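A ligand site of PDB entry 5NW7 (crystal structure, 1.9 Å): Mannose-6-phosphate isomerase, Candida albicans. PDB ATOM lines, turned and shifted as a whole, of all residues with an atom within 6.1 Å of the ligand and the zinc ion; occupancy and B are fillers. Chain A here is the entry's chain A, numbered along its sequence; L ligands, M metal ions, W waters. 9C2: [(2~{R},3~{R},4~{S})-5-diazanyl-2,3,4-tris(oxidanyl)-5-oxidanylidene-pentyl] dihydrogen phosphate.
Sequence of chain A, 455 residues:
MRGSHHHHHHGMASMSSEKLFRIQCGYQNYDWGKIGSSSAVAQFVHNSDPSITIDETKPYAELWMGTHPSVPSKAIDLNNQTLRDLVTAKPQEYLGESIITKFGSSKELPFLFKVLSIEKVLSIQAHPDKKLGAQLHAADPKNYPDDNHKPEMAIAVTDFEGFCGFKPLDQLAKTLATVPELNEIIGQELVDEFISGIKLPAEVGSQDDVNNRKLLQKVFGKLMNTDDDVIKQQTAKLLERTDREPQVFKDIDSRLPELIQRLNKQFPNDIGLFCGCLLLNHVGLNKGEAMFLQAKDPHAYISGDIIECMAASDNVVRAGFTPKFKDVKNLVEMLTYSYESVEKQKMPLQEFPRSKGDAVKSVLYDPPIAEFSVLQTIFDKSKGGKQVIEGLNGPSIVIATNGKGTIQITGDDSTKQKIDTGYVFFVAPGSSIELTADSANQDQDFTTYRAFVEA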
ATOM      1  N   TYR A  30      -5.468   6.545  20.437  1.00  0.00           N
ATOM      2  CA  TYR A  30      -4.548   6.807  19.362  1.00  0.00           C
ATOM      3  C   TYR A  30      -3.557   7.923  19.804  1.00  0.00           C
ATOM      4  O   TYR A  30      -3.900   8.808  20.583  1.00  0.00           O
ATOM      5  CB  TYR A  30      -5.292   7.263  18.099  1.00  0.00           C
ATOM      6  CG  TYR A  30      -6.333   6.297  17.528  1.00  0.00           C
ATOM      7  CD1 TYR A  30      -6.219   4.896  17.690  1.00  0.00           C
ATOM      8  CD2 TYR A  30      -7.413   6.815  16.746  1.00  0.00           C
ATOM      9  CE1 TYR A  30      -7.170   4.032  17.124  1.00  0.00           C
ATOM     10  CE2 TYR A  30      -8.362   5.960  16.177  1.00  0.00           C
ATOM     11  CZ  TYR A  30      -8.244   4.588  16.361  1.00  0.00           C
ATOM     12  OH  TYR A  30      -9.157   3.778  15.749  1.00  0.00           O
ATOM     13  N   TRP A  32      -2.353  10.630  18.654  1.00  0.00           N
ATOM     14  CA  TRP A  32      -2.677  12.035  18.485  1.00  0.00           C
ATOM     15  C   TRP A  32      -3.651  12.621  19.504  1.00  0.00           C
ATOM     16  O   TRP A  32      -3.904  13.830  19.516  1.00  0.00           O
ATOM     17  CB  TRP A  32      -3.143  12.294  17.065  1.00  0.00           C
ATOM     18  CG  TRP A  32      -4.252  11.400  16.618  1.00  0.00           C
ATOM     19  CD1 TRP A  32      -4.157  10.360  15.740  1.00  0.00           C
ATOM     20  CD2 TRP A  32      -5.604  11.579  16.899  1.00  0.00           C
ATOM     21  NE1 TRP A  32      -5.402   9.845  15.485  1.00  0.00           N
ATOM     22  CE2 TRP A  32      -6.320  10.573  16.202  1.00  0.00           C
ATOM     23  CE3 TRP A  32      -6.341  12.472  17.732  1.00  0.00           C
ATOM     24  CZ2 TRP A  32      -7.726  10.461  16.258  1.00  0.00           C
ATOM     25  CZ3 TRP A  32      -7.705  12.347  17.819  1.00  0.00           C
ATOM     26  CH2 TRP A  32      -8.404  11.328  17.061  1.00  0.00           C
ATOM     27  N   GLU A  62     -10.509   9.147  20.791  1.00  0.00           N
ATOM     28  CA  GLU A  62     -11.870   9.000  20.229  1.00  0.00           C
ATOM     29  C   GLU A  62     -12.790   8.283  21.198  1.00  0.00           C
ATOM     30  O   GLU A  62     -12.370   7.293  21.796  1.00  0.00           O
ATOM     31  CB  GLU A  62     -11.822   8.204  18.925  1.00  0.00           C
ATOM     32  CG  GLU A  62     -10.832   8.718  17.885  1.00  0.00           C
ATOM     33  CD  GLU A  62     -11.119   8.187  16.502  1.00  0.00           C
ATOM     34  OE1 GLU A  62     -11.786   7.120  16.354  1.00  0.00           O
ATOM     35  OE2 GLU A  62     -10.626   8.782  15.517  1.00  0.00           O
ATOM     36  N   TRP A  64     -16.265   6.211  20.920  1.00  0.00           N
ATOM     37  CA  TRP A  64     -17.118   5.601  19.871  1.00  0.00           C
ATOM     38  C   TRP A  64     -18.489   5.279  20.416  1.00  0.00           C
ATOM     39  O   TRP A  64     -18.592   4.618  21.425  1.00  0.00           O
ATOM     40  CB  TRP A  64     -16.495   4.294  19.317  1.00  0.00           C
ATOM     41  CG  TRP A  64     -15.314   4.473  18.424  1.00  0.00           C
ATOM     42  CD1 TRP A  64     -14.315   5.407  18.542  1.00  0.00           C
ATOM     43  CD2 TRP A  64     -14.962   3.661  17.318  1.00  0.00           C
ATOM     44  NE1 TRP A  64     -13.380   5.231  17.557  1.00  0.00           N
ATOM     45  CE2 TRP A  64     -13.750   4.146  16.806  1.00  0.00           C
ATOM     46  CE3 TRP A  64     -15.585   2.555  16.691  1.00  0.00           C
ATOM     47  CZ2 TRP A  64     -13.130   3.573  15.716  1.00  0.00           C
ATOM     48  CZ3 TRP A  64     -14.997   1.986  15.603  1.00  0.00           C
ATOM     49  CH2 TRP A  64     -13.759   2.481  15.122  1.00  0.00           C
ATOM     50  N   LYS A 114     -19.071   9.963  17.141  1.00  0.00           N
ATOM     51  CA  LYS A 114     -17.813  10.050  17.954  1.00  0.00           C
ATOM     52  C   LYS A 114     -17.614  11.405  18.617  1.00  0.00           C
ATOM     53  O   LYS A 114     -18.100  12.425  18.086  1.00  0.00           O
ATOM     54  CB  LYS A 114     -16.603   9.802  17.037  1.00  0.00           C
ATOM     55  CG  LYS A 114     -16.441   8.413  16.448  1.00  0.00           C
ATOM     56  CD  LYS A 114     -15.110   8.260  15.732  1.00  0.00           C
ATOM     57  CE  LYS A 114     -15.035   6.942  14.964  1.00  0.00           C
ATOM     58  NZ  LYS A 114     -13.638   6.816  14.484  1.00  0.00           N
ATOM     59  N   LEU A 116     -14.076  13.439  19.246  1.00  0.00           N
ATOM     60  CA  LEU A 116     -12.641  13.460  19.091  1.00  0.00           C
ATOM     61  C   LEU A 116     -12.013  14.539  19.943  1.00  0.00           C
ATOM     62  O   LEU A 116     -12.568  15.648  20.024  1.00  0.00           O
ATOM     63  CB  LEU A 116     -12.203  13.689  17.641  1.00  0.00           C
ATOM     64  CG  LEU A 116     -12.053  12.427  16.752  1.00  0.00           C
ATOM     65  CD1 LEU A 116     -13.326  11.662  16.568  1.00  0.00           C
ATOM     66  CD2 LEU A 116     -11.496  12.699  15.360  1.00  0.00           C
ATOM     67  N   LEU A 122      -4.042  14.551  12.761  1.00  0.00           N
ATOM     68  CA  LEU A 122      -4.297  13.170  12.306  1.00  0.00           C
ATOM     69  C   LEU A 122      -3.571  12.906  11.032  1.00  0.00           C
ATOM     70  O   LEU A 122      -2.995  13.811  10.448  1.00  0.00           O
ATOM     71  CB  LEU A 122      -5.802  12.787  12.151  1.00  0.00           C
ATOM     72  CG  LEU A 122      -6.894  13.268  13.122  1.00  0.00           C
ATOM     73  CD1 LEU A 122      -8.178  12.494  13.084  1.00  0.00           C
ATOM     74  CD2 LEU A 122      -6.483  13.609  14.567  1.00  0.00           C
ATOM     75  N   SER A 123      -3.606  11.633  10.600  1.00  0.00           N
ATOM     76  CA  SER A 123      -3.091  11.259   9.299  1.00  0.00           C
ATOM     77  C   SER A 123      -3.754  12.061   8.186  1.00  0.00           C
ATOM     78  O   SER A 123      -4.920  12.353   8.263  1.00  0.00           O
ATOM     79  CB  SER A 123      -3.244   9.755   9.031  1.00  0.00           C
ATOM     80  OG  SER A 123      -4.650   9.385   8.815  1.00  0.00           O
ATOM     81  N   ILE A 124      -2.939  12.393   7.194  1.00  0.00           N
ATOM     82  CA  ILE A 124      -3.392  12.731   5.846  1.00  0.00           C
ATOM     83  C   ILE A 124      -4.155  11.494   5.384  1.00  0.00           C
ATOM     84  O   ILE A 124      -3.561  10.396   5.224  1.00  0.00           O
ATOM     85  CB  ILE A 124      -2.194  13.028   4.872  1.00  0.00           C
ATOM     86  CG1 ILE A 124      -1.272  14.153   5.412  1.00  0.00           C
ATOM     87  CG2 ILE A 124      -2.743  13.375   3.497  1.00  0.00           C
ATOM     88  CD1 ILE A 124      -1.955  15.454   5.674  1.00  0.00           C
ATOM     89  N   GLN A 125      -5.444  11.647   5.196  1.00  0.00           N
ATOM     90  CA  GLN A 125      -6.324  10.522   5.016  1.00  0.00           C
ATOM     91  C   GLN A 125      -7.468  10.776   4.051  1.00  0.00           C
ATOM     92  O   GLN A 125      -7.898  11.920   3.786  1.00  0.00           O
ATOM     93  CB  GLN A 125      -6.843  10.041   6.344  1.00  0.00           C
ATOM     94  CG  GLN A 125      -7.900  10.941   6.944  1.00  0.00           C
ATOM     95  CD  GLN A 125      -8.279  10.605   8.378  1.00  0.00           C
ATOM     96  OE1 GLN A 125      -9.519  10.444   8.718  1.00  0.00           O
ATOM     97  NE2 GLN A 125      -7.255  10.642   9.236  1.00  0.00           N
ATOM     98  N   HIS A 127     -11.251   8.403   2.933  1.00  0.00           N
ATOM     99  CA  HIS A 127     -12.081   7.229   3.159  1.00  0.00           C
ATOM    100  C   HIS A 127     -12.697   6.788   1.807  1.00  0.00           C
ATOM    101  O   HIS A 127     -13.054   7.644   0.970  1.00  0.00           O
ATOM    102  CB  HIS A 127     -13.157   7.537   4.155  1.00  0.00           C
ATOM    103  CG  HIS A 127     -12.623   8.120   5.442  1.00  0.00           C
ATOM    104  ND1 HIS A 127     -11.801   7.412   6.291  1.00  0.00           N
ATOM    105  CD2 HIS A 127     -12.764   9.351   5.981  1.00  0.00           C
ATOM    106  CE1 HIS A 127     -11.476   8.188   7.325  1.00  0.00           C
ATOM    107  NE2 HIS A 127     -12.017   9.390   7.139  1.00  0.00           N
ATOM    108  N   LYS A 150     -17.221   5.859   3.804  1.00  0.00           N
ATOM    109  CA  LYS A 150     -17.271   6.725   5.005  1.00  0.00           C
ATOM    110  C   LYS A 150     -17.231   8.241   4.724  1.00  0.00           C
ATOM    111  O   LYS A 150     -16.321   8.946   5.107  1.00  0.00           O
ATOM    112  CB  LYS A 150     -16.223   6.321   6.007  1.00  0.00           C
ATOM    113  CG  LYS A 150     -16.507   6.792   7.422  1.00  0.00           C
ATOM    114  CD  LYS A 150     -15.347   6.515   8.387  1.00  0.00           C
ATOM    115  CE  LYS A 150     -14.608   7.789   8.711  1.00  0.00           C
ATOM    116  NZ  LYS A 150     -13.771   7.507   9.943  1.00  0.00           N
ATOM    117  N   GLU A 152     -18.275  11.716   6.136  1.00  0.00           N
ATOM    118  CA  GLU A 152     -18.342  12.136   7.547  1.00  0.00           C
ATOM    119  C   GLU A 152     -18.655  13.614   7.729  1.00  0.00           C
ATOM    120  O   GLU A 152     -18.607  14.427   6.776  1.00  0.00           O
ATOM    121  CB  GLU A 152     -17.029  11.791   8.211  1.00  0.00           C
ATOM    122  CG  GLU A 152     -15.813  12.464   7.658  1.00  0.00           C
ATOM    123  CD  GLU A 152     -14.528  12.193   8.461  1.00  0.00           C
ATOM    124  OE1 GLU A 152     -14.322  12.863   9.503  1.00  0.00           O
ATOM    125  OE2 GLU A 152     -13.661  11.398   8.018  1.00  0.00           O
ATOM    126  N   HIS A 299      -8.158  14.783   3.712  1.00  0.00           N
ATOM    127  CA  HIS A 299      -8.305  15.604   4.915  1.00  0.00           C
ATOM    128  C   HIS A 299      -7.385  15.174   6.053  1.00  0.00           C
ATOM    129  O   HIS A 299      -6.804  14.074   6.061  1.00  0.00           O
ATOM    130  CB  HIS A 299      -9.752  15.630   5.463  1.00  0.00           C
ATOM    131  CG  HIS A 299     -10.315  14.307   5.866  1.00  0.00           C
ATOM    132  ND1 HIS A 299     -10.715  13.361   4.934  1.00  0.00           N
ATOM    133  CD2 HIS A 299     -10.614  13.780   7.084  1.00  0.00           C
ATOM    134  CE1 HIS A 299     -11.226  12.310   5.570  1.00  0.00           C
ATOM    135  NE2 HIS A 299     -11.140  12.520   6.875  1.00  0.00           N
ATOM    136  N   TYR A 301      -7.454  16.373  10.350  1.00  0.00           N
ATOM    137  CA  TYR A 301      -7.876  17.284  11.445  1.00  0.00           C
ATOM    138  C   TYR A 301      -6.657  17.640  12.257  1.00  0.00           C
ATOM    139  O   TYR A 301      -5.802  16.754  12.505  1.00  0.00           O
ATOM    140  CB  TYR A 301      -9.003  16.645  12.290  1.00  0.00           C
ATOM    141  CG  TYR A 301     -10.323  16.365  11.487  1.00  0.00           C
ATOM    142  CD1 TYR A 301     -10.507  16.925  10.195  1.00  0.00           C
ATOM    143  CD2 TYR A 301     -11.344  15.529  11.957  1.00  0.00           C
ATOM    144  CE1 TYR A 301     -11.653  16.666   9.432  1.00  0.00           C
ATOM    145  CE2 TYR A 301     -12.489  15.262  11.172  1.00  0.00           C
ATOM    146  CZ  TYR A 301     -12.638  15.856   9.922  1.00  0.00           C
ATOM    147  OH  TYR A 301     -13.734  15.670   9.077  1.00  0.00           O
ATOM    148  N   GLU A 308     -18.065  14.143  15.799  1.00  0.00           N
ATOM    149  CA  GLU A 308     -17.991  13.631  14.460  1.00  0.00           C
ATOM    150  C   GLU A 308     -19.122  12.636  14.262  1.00  0.00           C
ATOM    151  O   GLU A 308     -19.529  11.885  15.189  1.00  0.00           O
ATOM    152  CB  GLU A 308     -16.615  13.029  14.282  1.00  0.00           C
ATOM    153  CG  GLU A 308     -16.000  12.922  12.917  1.00  0.00           C
ATOM    154  CD  GLU A 308     -14.620  12.249  13.013  1.00  0.00           C
ATOM    155  OE1 GLU A 308     -14.508  11.121  13.546  1.00  0.00           O
ATOM    156  OE2 GLU A 308     -13.612  12.872  12.630  1.00  0.00           O
ATOM    157  N   MET A 310     -20.440   9.753  11.075  1.00  0.00           N
ATOM    158  CA  MET A 310     -20.036   9.201   9.815  1.00  0.00           C
ATOM    159  C   MET A 310     -20.903   8.017   9.476  1.00  0.00           C
ATOM    160  O   MET A 310     -21.552   7.474  10.367  1.00  0.00           O
ATOM    161  CB  MET A 310     -18.583   8.739   9.923  1.00  0.00           C
ATOM    162  CG  MET A 310     -18.317   7.691  10.945  1.00  0.00           C
ATOM    163  SD  MET A 310     -16.807   7.977  11.922  1.00  0.00           S
ATOM    164  CE  MET A 310     -17.250   9.517  12.719  1.00  0.00           C
ATOM    165  N   ASP A 314     -14.776   1.864   9.542  1.00  0.00           N
ATOM    166  CA  ASP A 314     -13.488   2.311   9.972  1.00  0.00           C
ATOM    167  C   ASP A 314     -12.458   2.111   8.824  1.00  0.00           C
ATOM    168  O   ASP A 314     -11.300   1.826   9.058  1.00  0.00           O
ATOM    169  CB  ASP A 314     -13.043   1.574  11.246  1.00  0.00           C
ATOM    170  CG  ASP A 314     -11.940   2.355  11.998  1.00  0.00           C
ATOM    171  OD1 ASP A 314     -11.905   3.584  11.893  1.00  0.00           O
ATOM    172  OD2 ASP A 314     -11.135   1.707  12.685  1.00  0.00           O
ATOM    173  N   VAL A 316      -9.976   3.578   6.208  1.00  0.00           N
ATOM    174  CA  VAL A 316      -9.212   4.782   5.991  1.00  0.00           C
ATOM    175  C   VAL A 316      -7.925   4.492   5.270  1.00  0.00           C
ATOM    176  O   VAL A 316      -7.234   3.565   5.573  1.00  0.00           O
ATOM    177  CB  VAL A 316      -8.972   5.560   7.339  1.00  0.00           C
ATOM    178  CG1 VAL A 316      -8.218   4.721   8.342  1.00  0.00           C
ATOM    179  CG2 VAL A 316      -8.258   6.886   7.095  1.00  0.00           C
ATOM    180  N   ARG A 318      -4.359   6.129   4.544  1.00  0.00           N
ATOM    181  CA  ARG A 318      -3.532   7.173   5.166  1.00  0.00           C
ATOM    182  C   ARG A 318      -2.290   7.344   4.293  1.00  0.00           C
ATOM    183  O   ARG A 318      -1.830   6.383   3.715  1.00  0.00           O
ATOM    184  CB  ARG A 318      -3.069   6.738   6.541  1.00  0.00           C
ATOM    185  CG  ARG A 318      -4.203   6.278   7.434  1.00  0.00           C
ATOM    186  CD  ARG A 318      -3.679   5.983   8.827  1.00  0.00           C
ATOM    187  NE  ARG A 318      -4.666   5.308   9.630  1.00  0.00           N
ATOM    188  CZ  ARG A 318      -4.947   4.014   9.618  1.00  0.00           C
ATOM    189  NH1 ARG A 318      -4.337   3.141   8.815  1.00  0.00           N
ATOM    190  NH2 ARG A 318      -5.896   3.569  10.444  1.00  0.00           N
ATOM    191  N   PHE A 321       1.736  12.056   8.123  1.00  0.00           N
ATOM    192  CA  PHE A 321       1.560  12.440   9.528  1.00  0.00           C
ATOM    193  C   PHE A 321       1.005  11.283  10.392  1.00  0.00           C
ATOM    194  O   PHE A 321       0.081  11.479  11.170  1.00  0.00           O
ATOM    195  CB  PHE A 321       0.592  13.622   9.719  1.00  0.00           C
ATOM    196  CG  PHE A 321       1.022  14.936   9.174  1.00  0.00           C
ATOM    197  CD1 PHE A 321       2.294  15.445   9.418  1.00  0.00           C
ATOM    198  CD2 PHE A 321       0.078  15.770   8.616  1.00  0.00           C
ATOM    199  CE1 PHE A 321       2.643  16.759   9.059  1.00  0.00           C
ATOM    200  CE2 PHE A 321       0.431  17.053   8.174  1.00  0.00           C
ATOM    201  CZ  PHE A 321       1.722  17.558   8.411  1.00  0.00           C
ATOM    202  N   THR A 322       1.580  10.119  10.308  1.00  0.00           N
ATOM    203  CA  THR A 322       1.110   8.998  11.143  1.00  0.00           C
ATOM    204  C   THR A 322       2.160   7.864  11.220  1.00  0.00           C
ATOM    205  O   THR A 322       2.791   7.570  10.253  1.00  0.00           O
ATOM    206  CB  THR A 322      -0.250   8.385  10.594  1.00  0.00           C
ATOM    207  OG1 THR A 322      -0.726   7.330  11.433  1.00  0.00           O
ATOM    208  CG2 THR A 322      -0.059   7.775   9.187  1.00  0.00           C
ATOM    209  N   LYS A 324       0.798   4.900  11.746  1.00  0.00           N
ATOM    210  CA  LYS A 324      -0.090   3.780  11.373  1.00  0.00           C
ATOM    211  C   LYS A 324       0.157   3.405   9.920  1.00  0.00           C
ATOM    212  O   LYS A 324       0.994   4.039   9.234  1.00  0.00           O
ATOM    213  CB  LYS A 324      -1.581   4.139  11.591  1.00  0.00           C
ATOM    214  CG  LYS A 324      -1.958   4.568  13.017  1.00  0.00           C
ATOM    215  CD  LYS A 324      -3.380   5.147  13.005  1.00  0.00           C
ATOM    216  CE  LYS A 324      -4.044   5.096  14.364  1.00  0.00           C
ATOM    217  NZ  LYS A 324      -5.478   5.430  14.323  1.00  0.00           N
HETATM  218  O3  9C2 L   1     -10.994   7.476  13.331  1.00  0.00           O
HETATM  219  C4  9C2 L   1      -9.609   8.475  11.594  1.00  0.00           C
HETATM  220  C5  9C2 L   1      -8.642   8.895  12.733  1.00  0.00           C
HETATM  221  O4  9C2 L   1      -9.176   7.250  10.987  1.00  0.00           O
HETATM  222  N1  9C2 L   1     -11.541  11.600  11.049  1.00  0.00           N
HETATM  223  O5  9C2 L   1      -7.363   9.316  12.176  1.00  0.00           O
HETATM  224  O6  9C2 L   1      -4.942   9.016  11.472  1.00  0.00           O
HETATM  225  O7  9C2 L   1      -6.466   7.051  11.186  1.00  0.00           O
HETATM  226  O8  9C2 L   1      -5.847   7.785  13.556  1.00  0.00           O
HETATM  227  P   9C2 L   1      -6.121   8.264  12.080  1.00  0.00           P
HETATM  228  C3  9C2 L   1     -10.991   8.260  12.109  1.00  0.00           C
HETATM  229  C2  9C2 L   1     -11.750   9.568  12.312  1.00  0.00           C
HETATM  230  O2  9C2 L   1     -13.069   9.173  12.696  1.00  0.00           O
HETATM  231  C1  9C2 L   1     -11.803  10.321  11.023  1.00  0.00           C
HETATM  232  O1  9C2 L   1     -11.992   9.787   9.917  1.00  0.00           O
HETATM  233  N   9C2 L   1     -11.663  12.397   9.893  1.00  0.00           N
HETATM  234 ZN    ZN M   1     -11.673  11.142   8.340  1.00  0.00          ZN
HETATM  235  O   HOH W   1     -10.091   4.863  13.532  1.00  0.00           O
HETATM  236  O   HOH W   2      -8.461  13.498   9.521  1.00  0.00           O
HETATM  237  O   HOH W   3      -2.848   8.935  12.861  1.00  0.00           O
HETATM  238  O   HOH W   4      -7.331   4.676  12.508  1.00  0.00           O
HETATM  239  O   HOH W   5     -11.385   5.557   9.918  1.00  0.00           O
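Water W3 lies within hydrogen-bond range of an oxygen (O6) of the ligand (2.5 Å) and the side-chain hydroxyl of Thr 322 (3.0 Å).
Water W1 lies within hydrogen-bond range of OH of Tyr 30, OD1 of Asp 314 and O3 of the ligand.
Water W4 lies within hydrogen-bond range of the side-chain amino group (NZ) of Lys 324 (2.7 Å), the guanidinium group (NH2) of Arg 318 (2.7 Å) and an oxygen (O7) of the ligand (2.9 Å).
Water W5 lies within hydrogen-bond range of OD1 of Asp 314, O4 of the ligand and NZ of Lys 150.
Water W2 bridges NE2 of Gln 125 (3.1 Å) and N of Tyr 301 (3.2 Å).
The zinc ion is bound by N of the ligand (2.0 Å), OE2 of Glu 152 (2.0 Å), NE2 of His 299 (2.1 Å), O1 of the ligand (2.1 Å), NE2 of His 127 (2.2 Å) and OE1 of Gln 125 (2.3 Å).
The zinc ion has six donor atoms within binding distance.
The backbone NH (N) of Lys 114 lies within hydrogen-bond range of the backbone carbonyl oxygen (O) of Glu 308, 2.8 Å away.
The side-chain amide nitrogen (NE2) of Gln 125 lies within hydrogen-bond range of the side-chain hydroxyl (OG) of Ser 123 (2.9 Å).
O of Tyr 301 sits at hydrogen-bond distance from N of Leu 122 (2.8 Å).
The side-chain carboxylate (OE1) of Glu 62 is in salt-bridge range of the side-chain amino group (NZ) of Lys 114 (2.6 Å).
OE1 of Glu 62 lies within hydrogen-bond range of NE1 of Trp 64 (2.7 Å).
The side-chain amino group (NZ) of Lys 150 is in hydrogen-bond range of the side-chain sulfur (SD) of Met 310.
The side-chain carboxylate of Glu 152 is in hydrogen-bond range of the side-chain hydroxyl of Tyr 301 (2.9 Å).
The side-chain hydroxyl (OG1) of Thr 322 is in hydrogen-bond range of the backbone NH (N) of Lys 324, 2.9 Å away.
Of the 23 residues printed, 4 come within 4 Å of the zinc ion.
CD2 of Tyr 30 touches O8 of the ligand (3.7 Å).
Leu 122 touches the ligand.
CE2 of Tyr 301 touches N of the ligand, at 3.2 Å.
Val 316 touches the ligand.
Hydrophobic or aromatic side chains within 4 Å of the ligand: Tyr 30, Trp 32, Leu 122, His 127, His 299, Tyr 301 and Val 316.
Within 4 Å of the ligand: Tyr 30, Trp 32, Glu 62, Lys 114, Leu 122, Ser 123, Gln 125, His 127, Lys 150, Glu 152, His 299, Tyr 301, Glu 308, Val 316, Arg 318 and Lys 324.
O3 of the ligand lies within hydrogen-bond range of OE2 of Glu 62.
The guanidinium group of Arg 318 is in salt-bridge range of an oxygen (O7) of the ligand (2.9 Å).
The backbone NH (N) of Ser 123 sits close to an oxygen (O6) of the ligand (3.1 Å).
NZ of Lys 324 is in salt-bridge range of O8 of the ligand (2.5 Å).
The side-chain carboxylate of Glu 308 lies within hydrogen-bond range of an oxygen (O2) of the ligand, 2.6 Å away.
The indole nitrogen (NE1) of Trp 32 lies within hydrogen-bond range of an oxygen (O8) of the ligand, at 2.9 Å.
O2 of the ligand is in hydrogen-bond range of NZ of Lys 150 (3.3 Å).
O3 of the ligand is in hydrogen-bond range of NZ of Lys 114 (3.0 Å).
O6 of the ligand is in hydrogen-bond range of OG of Ser 123, at 2.7 Å.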
